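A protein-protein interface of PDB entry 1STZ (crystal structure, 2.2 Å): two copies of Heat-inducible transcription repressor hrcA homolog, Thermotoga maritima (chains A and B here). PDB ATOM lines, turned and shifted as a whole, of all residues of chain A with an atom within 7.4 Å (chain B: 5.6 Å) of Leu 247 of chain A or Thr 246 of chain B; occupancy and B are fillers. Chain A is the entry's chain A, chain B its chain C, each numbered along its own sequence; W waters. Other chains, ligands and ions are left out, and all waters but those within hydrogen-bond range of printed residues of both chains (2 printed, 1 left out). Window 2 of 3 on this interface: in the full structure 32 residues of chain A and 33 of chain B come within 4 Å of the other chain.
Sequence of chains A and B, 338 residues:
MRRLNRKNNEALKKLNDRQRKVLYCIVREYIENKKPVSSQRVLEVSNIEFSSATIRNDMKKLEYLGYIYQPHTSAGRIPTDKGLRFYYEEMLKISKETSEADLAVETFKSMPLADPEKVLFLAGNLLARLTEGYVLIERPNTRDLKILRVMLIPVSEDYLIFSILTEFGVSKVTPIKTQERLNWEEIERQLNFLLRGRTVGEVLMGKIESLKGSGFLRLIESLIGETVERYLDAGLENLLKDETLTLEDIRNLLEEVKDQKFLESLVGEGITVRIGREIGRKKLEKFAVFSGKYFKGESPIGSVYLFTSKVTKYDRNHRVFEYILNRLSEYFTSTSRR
Of the 11 printed residues of chain B, 7 touch a printed residue of chain A. Printed residues of chain B that touch a printed residue of chain A: Leu 240, Asp 242, Leu 245, Thr 246, Leu 247, Ile 250 and Arg 251. Printed residues of chain A that touch a printed residue of chain B: Leu 240, Leu 245, Leu 247, Ile 250 and Arg 251. Hydrophobic or aromatic side chains of chain A within 4 Å of the printed part of chain B: Leu 240, Leu 247 and Ile 250. Among the printed residues, 13 pairs touch across the chains.
Of chain B, only Leu 240 (3.7 Å), Leu 245 (3.5 Å), Thr 246 (3.8 Å) and Leu 247 (3.7 Å) come within 4 Å of Leu 247 of chain A. Printed residues of chain A within 4 Å of Asp 242 of chain B: Arg 251. Of the printed residues of chain A, Leu 245 of chain B touches Leu 247 (3.5 Å) and Arg 251 (3.9 Å). Of the printed residues of chain A, Leu 247 of chain B touches Leu 240, Leu 245 and Leu 247. The nearest residue of chain B that does not touch Leu 247 of chain A is Ile 250 of chain B (5.1 Å). The nearest residue of chain A that does not touch Thr 246 of chain B is Arg 251 of chain A (6.1 Å).
Among the printed residues, merely in contact across the chains: Leu 247 of chain A with Leu 245 of chain B, Leu 240 of chain A with Leu 240 of chain B, Leu 247 of chain A with Leu 247 of chain B, Leu 245 of chain A with Leu 247 of chain B, Leu 247 of chain A with Leu 240 of chain B, Leu 247 of chain A with Thr 246 of chain B, Ile 250 of chain A with Leu 240 of chain B, Arg 251 of chain A with Leu 245 of chain B, Leu 240 of chain A with Ile 250 of chain B and Leu 240 of chain A with Leu 247 of chain B.
O of Leu 240 of chain A is in hydrogen-bond range of NE of Arg 251 of chain B, at 2.8 Å. The guanidinium group (NE) of Arg 251 of chain A sits at hydrogen-bond distance from the backbone carbonyl oxygen (O) of Leu 240 of chain B (2.6 Å). NH2 of Arg 251 of chain A lies within hydrogen-bond range of O of Asp 242 of chain B (3.2 Å).
The side-chain carboxylate (OE1) of Glu 248 of chain A is in salt-bridge range of the guanidinium group (NH1) of Arg 251 of chain A (3.3 Å). The side-chain carboxylate (OD1) of Asp 242 of chain B sits at hydrogen-bond distance from the side-chain hydroxyl (OG1) of Thr 244 of chain B (2.4 Å). N of Glu 248 of chain B lies close to OG1 of Thr 246 of chain B. The backbone NH of Asp 249 of chain B lies within hydrogen-bond range of the side-chain hydroxyl of Thr 246 of chain B, 3.1 Å away.
Leu 240 of chain A touches Leu 247 of chain B, and with the chains exchanged Leu 247 of chain A touches Leu 240 of chain B. Leu 240 of chain A touches Arg 251 of chain B, and with the chains exchanged Arg 251 of chain A touches Leu 240 of chain B. Leu 247 of chain A touches Thr 246 of chain B, but with the chains exchanged Thr 246 of chain A does not touch Leu 247 of chain B (4.3 Å). Leu 247 of chain A touches its own counterpart, Leu 247 of chain B. Positions printed for both chains: 240, 245, 246, 247, 248, 249, 250 and 251. Of the 13 pairs that touch across the chains among the printed residues, 10 have their exchanged pair printed and touching as well.
Water W2 lies within hydrogen-bond range of the backbone carbonyl oxygen of Leu 245 of chain A (2.6 Å) and the guanidinium group of Arg 251 of chain B (3.4 Å). Water W1 lies within hydrogen-bond range of NH2 of Arg 251 of chain B (2.9 Å), O of Leu 240 of chain A (3.1 Å) and O of Leu 245 of chain A (3.2 Å).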
ATOM      1  N   LEU A 240     -31.306  15.115 -28.037  1.00  0.00           N
ATOM      2  CA  LEU A 240     -31.358  16.578 -28.113  1.00  0.00           C
ATOM      3  C   LEU A 240     -32.767  17.172 -28.026  1.00  0.00           C
ATOM      4  O   LEU A 240     -32.922  18.348 -27.697  1.00  0.00           O
ATOM      5  CB  LEU A 240     -30.729  17.053 -29.416  1.00  0.00           C
ATOM      6  CG  LEU A 240     -29.323  16.576 -29.742  1.00  0.00           C
ATOM      7  CD1 LEU A 240     -29.018  16.927 -31.186  1.00  0.00           C
ATOM      8  CD2 LEU A 240     -28.337  17.236 -28.812  1.00  0.00           C
ATOM      9  N   LEU A 245     -32.718  16.377 -20.541  1.00  0.00           N
ATOM     10  CA  LEU A 245     -31.286  16.135 -20.695  1.00  0.00           C
ATOM     11  C   LEU A 245     -30.578  17.440 -21.029  1.00  0.00           C
ATOM     12  O   LEU A 245     -31.131  18.303 -21.731  1.00  0.00           O
ATOM     13  CB  LEU A 245     -31.031  15.087 -21.792  1.00  0.00           C
ATOM     14  CG  LEU A 245     -31.555  13.672 -21.563  1.00  0.00           C
ATOM     15  CD1 LEU A 245     -31.345  12.788 -22.804  1.00  0.00           C
ATOM     16  CD2 LEU A 245     -30.914  13.026 -20.334  1.00  0.00           C
ATOM     17  N   THR A 246     -29.362  17.609 -20.519  1.00  0.00           N
ATOM     18  CA  THR A 246     -28.572  18.798 -20.818  1.00  0.00           C
ATOM     19  C   THR A 246     -27.500  18.448 -21.838  1.00  0.00           C
ATOM     20  O   THR A 246     -27.248  17.282 -22.108  1.00  0.00           O
ATOM     21  CB  THR A 246     -27.883  19.351 -19.559  1.00  0.00           C
ATOM     22  OG1 THR A 246     -26.982  18.365 -19.040  1.00  0.00           O
ATOM     23  CG2 THR A 246     -28.894  19.632 -18.419  1.00  0.00           C
ATOM     24  N   LEU A 247     -26.870  19.482 -22.360  1.00  0.00           N
ATOM     25  CA  LEU A 247     -25.734  19.376 -23.263  1.00  0.00           C
ATOM     26  C   LEU A 247     -24.619  18.560 -22.628  1.00  0.00           C
ATOM     27  O   LEU A 247     -24.041  17.693 -23.275  1.00  0.00           O
ATOM     28  CB  LEU A 247     -25.209  20.765 -23.616  1.00  0.00           C
ATOM     29  CG  LEU A 247     -24.637  21.021 -25.002  1.00  0.00           C
ATOM     30  CD1 LEU A 247     -23.896  22.360 -25.037  1.00  0.00           C
ATOM     31  CD2 LEU A 247     -23.739  19.912 -25.452  1.00  0.00           C
ATOM     32  N   GLU A 248     -24.326  18.831 -21.362  1.00  0.00           N
ATOM     33  CA  GLU A 248     -23.303  18.067 -20.645  1.00  0.00           C
ATOM     34  C   GLU A 248     -23.670  16.588 -20.473  1.00  0.00           C
ATOM     35  O   GLU A 248     -22.815  15.736 -20.636  1.00  0.00           O
ATOM     36  CB  GLU A 248     -22.953  18.712 -19.279  1.00  0.00           C
ATOM     37  CG  GLU A 248     -21.444  18.808 -19.003  1.00  0.00           C
ATOM     38  CD  GLU A 248     -20.776  20.068 -19.540  1.00  0.00           C
ATOM     39  OE1 GLU A 248     -20.251  20.047 -20.697  1.00  0.00           O
ATOM     40  OE2 GLU A 248     -20.740  21.089 -18.781  1.00  0.00           O
ATOM     41  N   ASP A 249     -24.922  16.267 -20.158  1.00  0.00           N
ATOM     42  CA  ASP A 249     -25.329  14.870 -20.091  1.00  0.00           C
ATOM     43  C   ASP A 249     -24.988  14.174 -21.406  1.00  0.00           C
ATOM     44  O   ASP A 249     -24.446  13.070 -21.401  1.00  0.00           O
ATOM     45  CB  ASP A 249     -26.830  14.697 -19.858  1.00  0.00           C
ATOM     46  CG  ASP A 249     -27.293  15.177 -18.478  1.00  0.00           C
ATOM     47  OD1 ASP A 249     -26.518  15.082 -17.484  1.00  0.00           O
ATOM     48  OD2 ASP A 249     -28.449  15.644 -18.304  1.00  0.00           O
ATOM     49  N   ILE A 250     -25.303  14.831 -22.516  1.00  0.00           N
ATOM     50  CA  ILE A 250     -25.138  14.233 -23.827  1.00  0.00           C
ATOM     51  C   ILE A 250     -23.666  14.062 -24.222  1.00  0.00           C
ATOM     52  O   ILE A 250     -23.280  12.995 -24.711  1.00  0.00           O
ATOM     53  CB  ILE A 250     -25.921  15.024 -24.897  1.00  0.00           C
ATOM     54  CG1 ILE A 250     -27.426  14.942 -24.603  1.00  0.00           C
ATOM     55  CG2 ILE A 250     -25.662  14.440 -26.281  1.00  0.00           C
ATOM     56  CD1 ILE A 250     -28.265  15.965 -25.350  1.00  0.00           C
ATOM     57  N   ARG A 251     -22.862  15.088 -24.004  1.00  0.00           N
ATOM     58  CA  ARG A 251     -21.415  14.981 -24.178  1.00  0.00           C
ATOM     59  C   ARG A 251     -20.876  13.839 -23.312  1.00  0.00           C
ATOM     60  O   ARG A 251     -20.073  13.050 -23.771  1.00  0.00           O
ATOM     61  CB  ARG A 251     -20.710  16.263 -23.786  1.00  0.00           C
ATOM     62  CG  ARG A 251     -20.900  17.409 -24.737  1.00  0.00           C
ATOM     63  CD  ARG A 251     -20.395  18.717 -24.181  1.00  0.00           C
ATOM     64  NE  ARG A 251     -20.350  19.750 -25.197  1.00  0.00           N
ATOM     65  CZ  ARG A 251     -20.276  21.048 -24.944  1.00  0.00           C
ATOM     66  NH1 ARG A 251     -20.196  21.508 -23.706  1.00  0.00           N
ATOM     67  NH2 ARG A 251     -20.241  21.907 -25.949  1.00  0.00           N
ATOM     68  N   ASN A 252     -21.343  13.739 -22.070  1.00  0.00           N
ATOM     69  CA  ASN A 252     -20.873  12.670 -21.172  1.00  0.00           C
ATOM     70  C   ASN A 252     -21.183  11.302 -21.745  1.00  0.00           C
ATOM     71  O   ASN A 252     -20.363  10.412 -21.685  1.00  0.00           O
ATOM     72  CB  ASN A 252     -21.469  12.786 -19.768  1.00  0.00           C
ATOM     73  CG  ASN A 252     -20.898  13.956 -18.986  1.00  0.00           C
ATOM     74  OD1 ASN A 252     -19.811  14.433 -19.277  1.00  0.00           O
ATOM     75  ND2 ASN A 252     -21.643  14.418 -17.980  1.00  0.00           N
ATOM     76  N   LEU A 253     -22.361  11.141 -22.319  1.00  0.00           N
ATOM     77  CA  LEU A 253     -22.756   9.863 -22.873  1.00  0.00           C
ATOM     78  C   LEU A 253     -21.854   9.492 -24.049  1.00  0.00           C
ATOM     79  O   LEU A 253     -21.344   8.371 -24.116  1.00  0.00           O
ATOM     80  CB  LEU A 253     -24.194   9.915 -23.338  1.00  0.00           C
ATOM     81  CG  LEU A 253     -25.090   8.671 -23.373  1.00  0.00           C
ATOM     82  CD1 LEU A 253     -25.651   8.494 -24.713  1.00  0.00           C
ATOM     83  CD2 LEU A 253     -24.445   7.396 -22.879  1.00  0.00           C
ATOM     84  N   LEU A 254     -21.659  10.443 -24.961  1.00  0.00           N
ATOM     85  CA  LEU A 254     -20.906  10.189 -26.180  1.00  0.00           C
ATOM     86  C   LEU A 254     -19.469   9.821 -25.827  1.00  0.00           C
ATOM     87  O   LEU A 254     -18.888   8.977 -26.460  1.00  0.00           O
ATOM     88  CB  LEU A 254     -20.931  11.404 -27.101  1.00  0.00           C
ATOM     89  CG  LEU A 254     -22.318  11.665 -27.688  1.00  0.00           C
ATOM     90  CD1 LEU A 254     -22.370  13.029 -28.397  1.00  0.00           C
ATOM     91  CD2 LEU A 254     -22.738  10.535 -28.624  1.00  0.00           C
ATOM     92  N   LEU B 240     -21.852  18.921 -31.063  1.00  0.00           N
ATOM     93  CA  LEU B 240     -22.000  18.705 -29.627  1.00  0.00           C
ATOM     94  C   LEU B 240     -20.704  18.841 -28.842  1.00  0.00           C
ATOM     95  O   LEU B 240     -20.757  19.031 -27.643  1.00  0.00           O
ATOM     96  CB  LEU B 240     -22.665  17.351 -29.341  1.00  0.00           C
ATOM     97  CG  LEU B 240     -24.184  17.411 -29.534  1.00  0.00           C
ATOM     98  CD1 LEU B 240     -24.727  16.159 -30.169  1.00  0.00           C
ATOM     99  CD2 LEU B 240     -24.866  17.673 -28.216  1.00  0.00           C
ATOM    100  N   ASP B 242     -18.300  21.188 -29.713  1.00  0.00           N
ATOM    101  CA  ASP B 242     -17.840  22.556 -29.884  1.00  0.00           C
ATOM    102  C   ASP B 242     -18.282  23.407 -28.690  1.00  0.00           C
ATOM    103  O   ASP B 242     -19.471  23.623 -28.478  1.00  0.00           O
ATOM    104  CB  ASP B 242     -18.418  23.115 -31.186  1.00  0.00           C
ATOM    105  CG  ASP B 242     -17.631  24.274 -31.718  1.00  0.00           C
ATOM    106  OD1 ASP B 242     -17.170  25.114 -30.902  1.00  0.00           O
ATOM    107  OD2 ASP B 242     -17.430  24.429 -32.945  1.00  0.00           O
ATOM    108  N   THR B 244     -18.300  26.463 -28.101  1.00  0.00           N
ATOM    109  CA  THR B 244     -19.017  27.697 -28.431  1.00  0.00           C
ATOM    110  C   THR B 244     -20.509  27.548 -28.698  1.00  0.00           C
ATOM    111  O   THR B 244     -21.208  28.551 -28.754  1.00  0.00           O
ATOM    112  CB  THR B 244     -18.368  28.398 -29.631  1.00  0.00           C
ATOM    113  OG1 THR B 244     -17.893  27.428 -30.578  1.00  0.00           O
ATOM    114  CG2 THR B 244     -17.120  29.147 -29.183  1.00  0.00           C
ATOM    115  N   LEU B 245     -21.000  26.320 -28.864  1.00  0.00           N
ATOM    116  CA  LEU B 245     -22.408  26.095 -29.163  1.00  0.00           C
ATOM    117  C   LEU B 245     -23.145  25.542 -27.954  1.00  0.00           C
ATOM    118  O   LEU B 245     -22.613  24.715 -27.210  1.00  0.00           O
ATOM    119  CB  LEU B 245     -22.559  25.127 -30.347  1.00  0.00           C
ATOM    120  CG  LEU B 245     -21.944  25.576 -31.665  1.00  0.00           C
ATOM    121  CD1 LEU B 245     -22.053  24.473 -32.697  1.00  0.00           C
ATOM    122  CD2 LEU B 245     -22.622  26.841 -32.152  1.00  0.00           C
ATOM    123  N   THR B 246     -24.380  25.993 -27.771  1.00  0.00           N
ATOM    124  CA  THR B 246     -25.243  25.471 -26.716  1.00  0.00           C
ATOM    125  C   THR B 246     -26.252  24.504 -27.306  1.00  0.00           C
ATOM    126  O   THR B 246     -26.399  24.384 -28.525  1.00  0.00           O
ATOM    127  CB  THR B 246     -26.030  26.598 -26.057  1.00  0.00           C
ATOM    128  OG1 THR B 246     -26.915  27.169 -27.030  1.00  0.00           O
ATOM    129  CG2 THR B 246     -25.102  27.751 -25.609  1.00  0.00           C
ATOM    130  N   LEU B 247     -26.976  23.862 -26.402  1.00  0.00           N
ATOM    131  CA  LEU B 247     -28.058  22.957 -26.751  1.00  0.00           C
ATOM    132  C   LEU B 247     -29.130  23.706 -27.542  1.00  0.00           C
ATOM    133  O   LEU B 247     -29.672  23.172 -28.503  1.00  0.00           O
ATOM    134  CB  LEU B 247     -28.663  22.355 -25.487  1.00  0.00           C
ATOM    135  CG  LEU B 247     -29.081  20.889 -25.511  1.00  0.00           C
ATOM    136  CD1 LEU B 247     -30.107  20.644 -24.405  1.00  0.00           C
ATOM    137  CD2 LEU B 247     -29.617  20.450 -26.841  1.00  0.00           C
ATOM    138  N   GLU B 248     -29.416  24.935 -27.105  1.00  0.00           N
ATOM    139  CA  GLU B 248     -30.371  25.838 -27.758  1.00  0.00           C
ATOM    140  C   GLU B 248     -29.986  26.095 -29.211  1.00  0.00           C
ATOM    141  O   GLU B 248     -30.824  26.016 -30.095  1.00  0.00           O
ATOM    142  CB  GLU B 248     -30.452  27.186 -27.003  1.00  0.00           C
ATOM    143  CG  GLU B 248     -31.858  27.786 -26.850  1.00  0.00           C
ATOM    144  CD  GLU B 248     -31.848  29.304 -26.594  1.00  0.00           C
ATOM    145  OE1 GLU B 248     -30.849  29.990 -26.907  1.00  0.00           O
ATOM    146  OE2 GLU B 248     -32.853  29.828 -26.082  1.00  0.00           O
ATOM    147  N   ASP B 249     -28.714  26.388 -29.452  1.00  0.00           N
ATOM    148  CA  ASP B 249     -28.228  26.643 -30.805  1.00  0.00           C
ATOM    149  C   ASP B 249     -28.393  25.421 -31.696  1.00  0.00           C
ATOM    150  O   ASP B 249     -28.822  25.534 -32.845  1.00  0.00           O
ATOM    151  CB  ASP B 249     -26.742  27.017 -30.817  1.00  0.00           C
ATOM    152  CG  ASP B 249     -26.441  28.356 -30.145  1.00  0.00           C
ATOM    153  OD1 ASP B 249     -27.268  29.307 -30.193  1.00  0.00           O
ATOM    154  OD2 ASP B 249     -25.347  28.554 -29.568  1.00  0.00           O
ATOM    155  N   ILE B 250     -28.025  24.256 -31.171  1.00  0.00           N
ATOM    156  CA  ILE B 250     -28.068  23.039 -31.958  1.00  0.00           C
ATOM    157  C   ILE B 250     -29.532  22.676 -32.247  1.00  0.00           C
ATOM    158  O   ILE B 250     -29.852  22.312 -33.367  1.00  0.00           O
ATOM    159  CB  ILE B 250     -27.316  21.892 -31.245  1.00  0.00           C
ATOM    160  CG1 ILE B 250     -25.809  22.195 -31.229  1.00  0.00           C
ATOM    161  CG2 ILE B 250     -27.586  20.563 -31.934  1.00  0.00           C
ATOM    162  CD1 ILE B 250     -25.031  21.378 -30.216  1.00  0.00           C
ATOM    163  N   ARG B 251     -30.413  22.820 -31.263  1.00  0.00           N
ATOM    164  CA  ARG B 251     -31.840  22.592 -31.494  1.00  0.00           C
ATOM    165  C   ARG B 251     -32.385  23.487 -32.603  1.00  0.00           C
ATOM    166  O   ARG B 251     -33.093  23.023 -33.487  1.00  0.00           O
ATOM    167  CB  ARG B 251     -32.651  22.840 -30.230  1.00  0.00           C
ATOM    168  CG  ARG B 251     -32.650  21.702 -29.244  1.00  0.00           C
ATOM    169  CD  ARG B 251     -33.199  22.099 -27.897  1.00  0.00           C
ATOM    170  NE  ARG B 251     -33.186  20.985 -26.960  1.00  0.00           N
ATOM    171  CZ  ARG B 251     -33.523  21.090 -25.685  1.00  0.00           C
ATOM    172  NH1 ARG B 251     -33.869  22.262 -25.171  1.00  0.00           N
ATOM    173  NH2 ARG B 251     -33.501  20.016 -24.912  1.00  0.00           N
ATOM    174  N   LYS B 286     -24.874  31.930 -33.945  1.00  0.00           N
ATOM    175  CA  LYS B 286     -23.619  31.354 -33.489  1.00  0.00           C
ATOM    176  C   LYS B 286     -22.955  30.474 -34.542  1.00  0.00           C
ATOM    177  O   LYS B 286     -21.894  29.919 -34.272  1.00  0.00           O
ATOM    178  CB  LYS B 286     -23.820  30.549 -32.202  1.00  0.00           C
ATOM    179  CG  LYS B 286     -24.490  31.321 -31.057  1.00  0.00           C
ATOM    180  CD  LYS B 286     -23.490  32.056 -30.142  1.00  0.00           C
ATOM    181  CE  LYS B 286     -22.832  31.167 -29.038  1.00  0.00           C
ATOM    182  NZ  LYS B 286     -23.527  29.880 -28.609  1.00  0.00           N
HETATM  183  O   HOH W   1     -31.754  17.747 -24.865  1.00  0.00           O
HETATM  184  O   HOH W   2     -32.453  20.538 -21.753  1.00  0.00           O
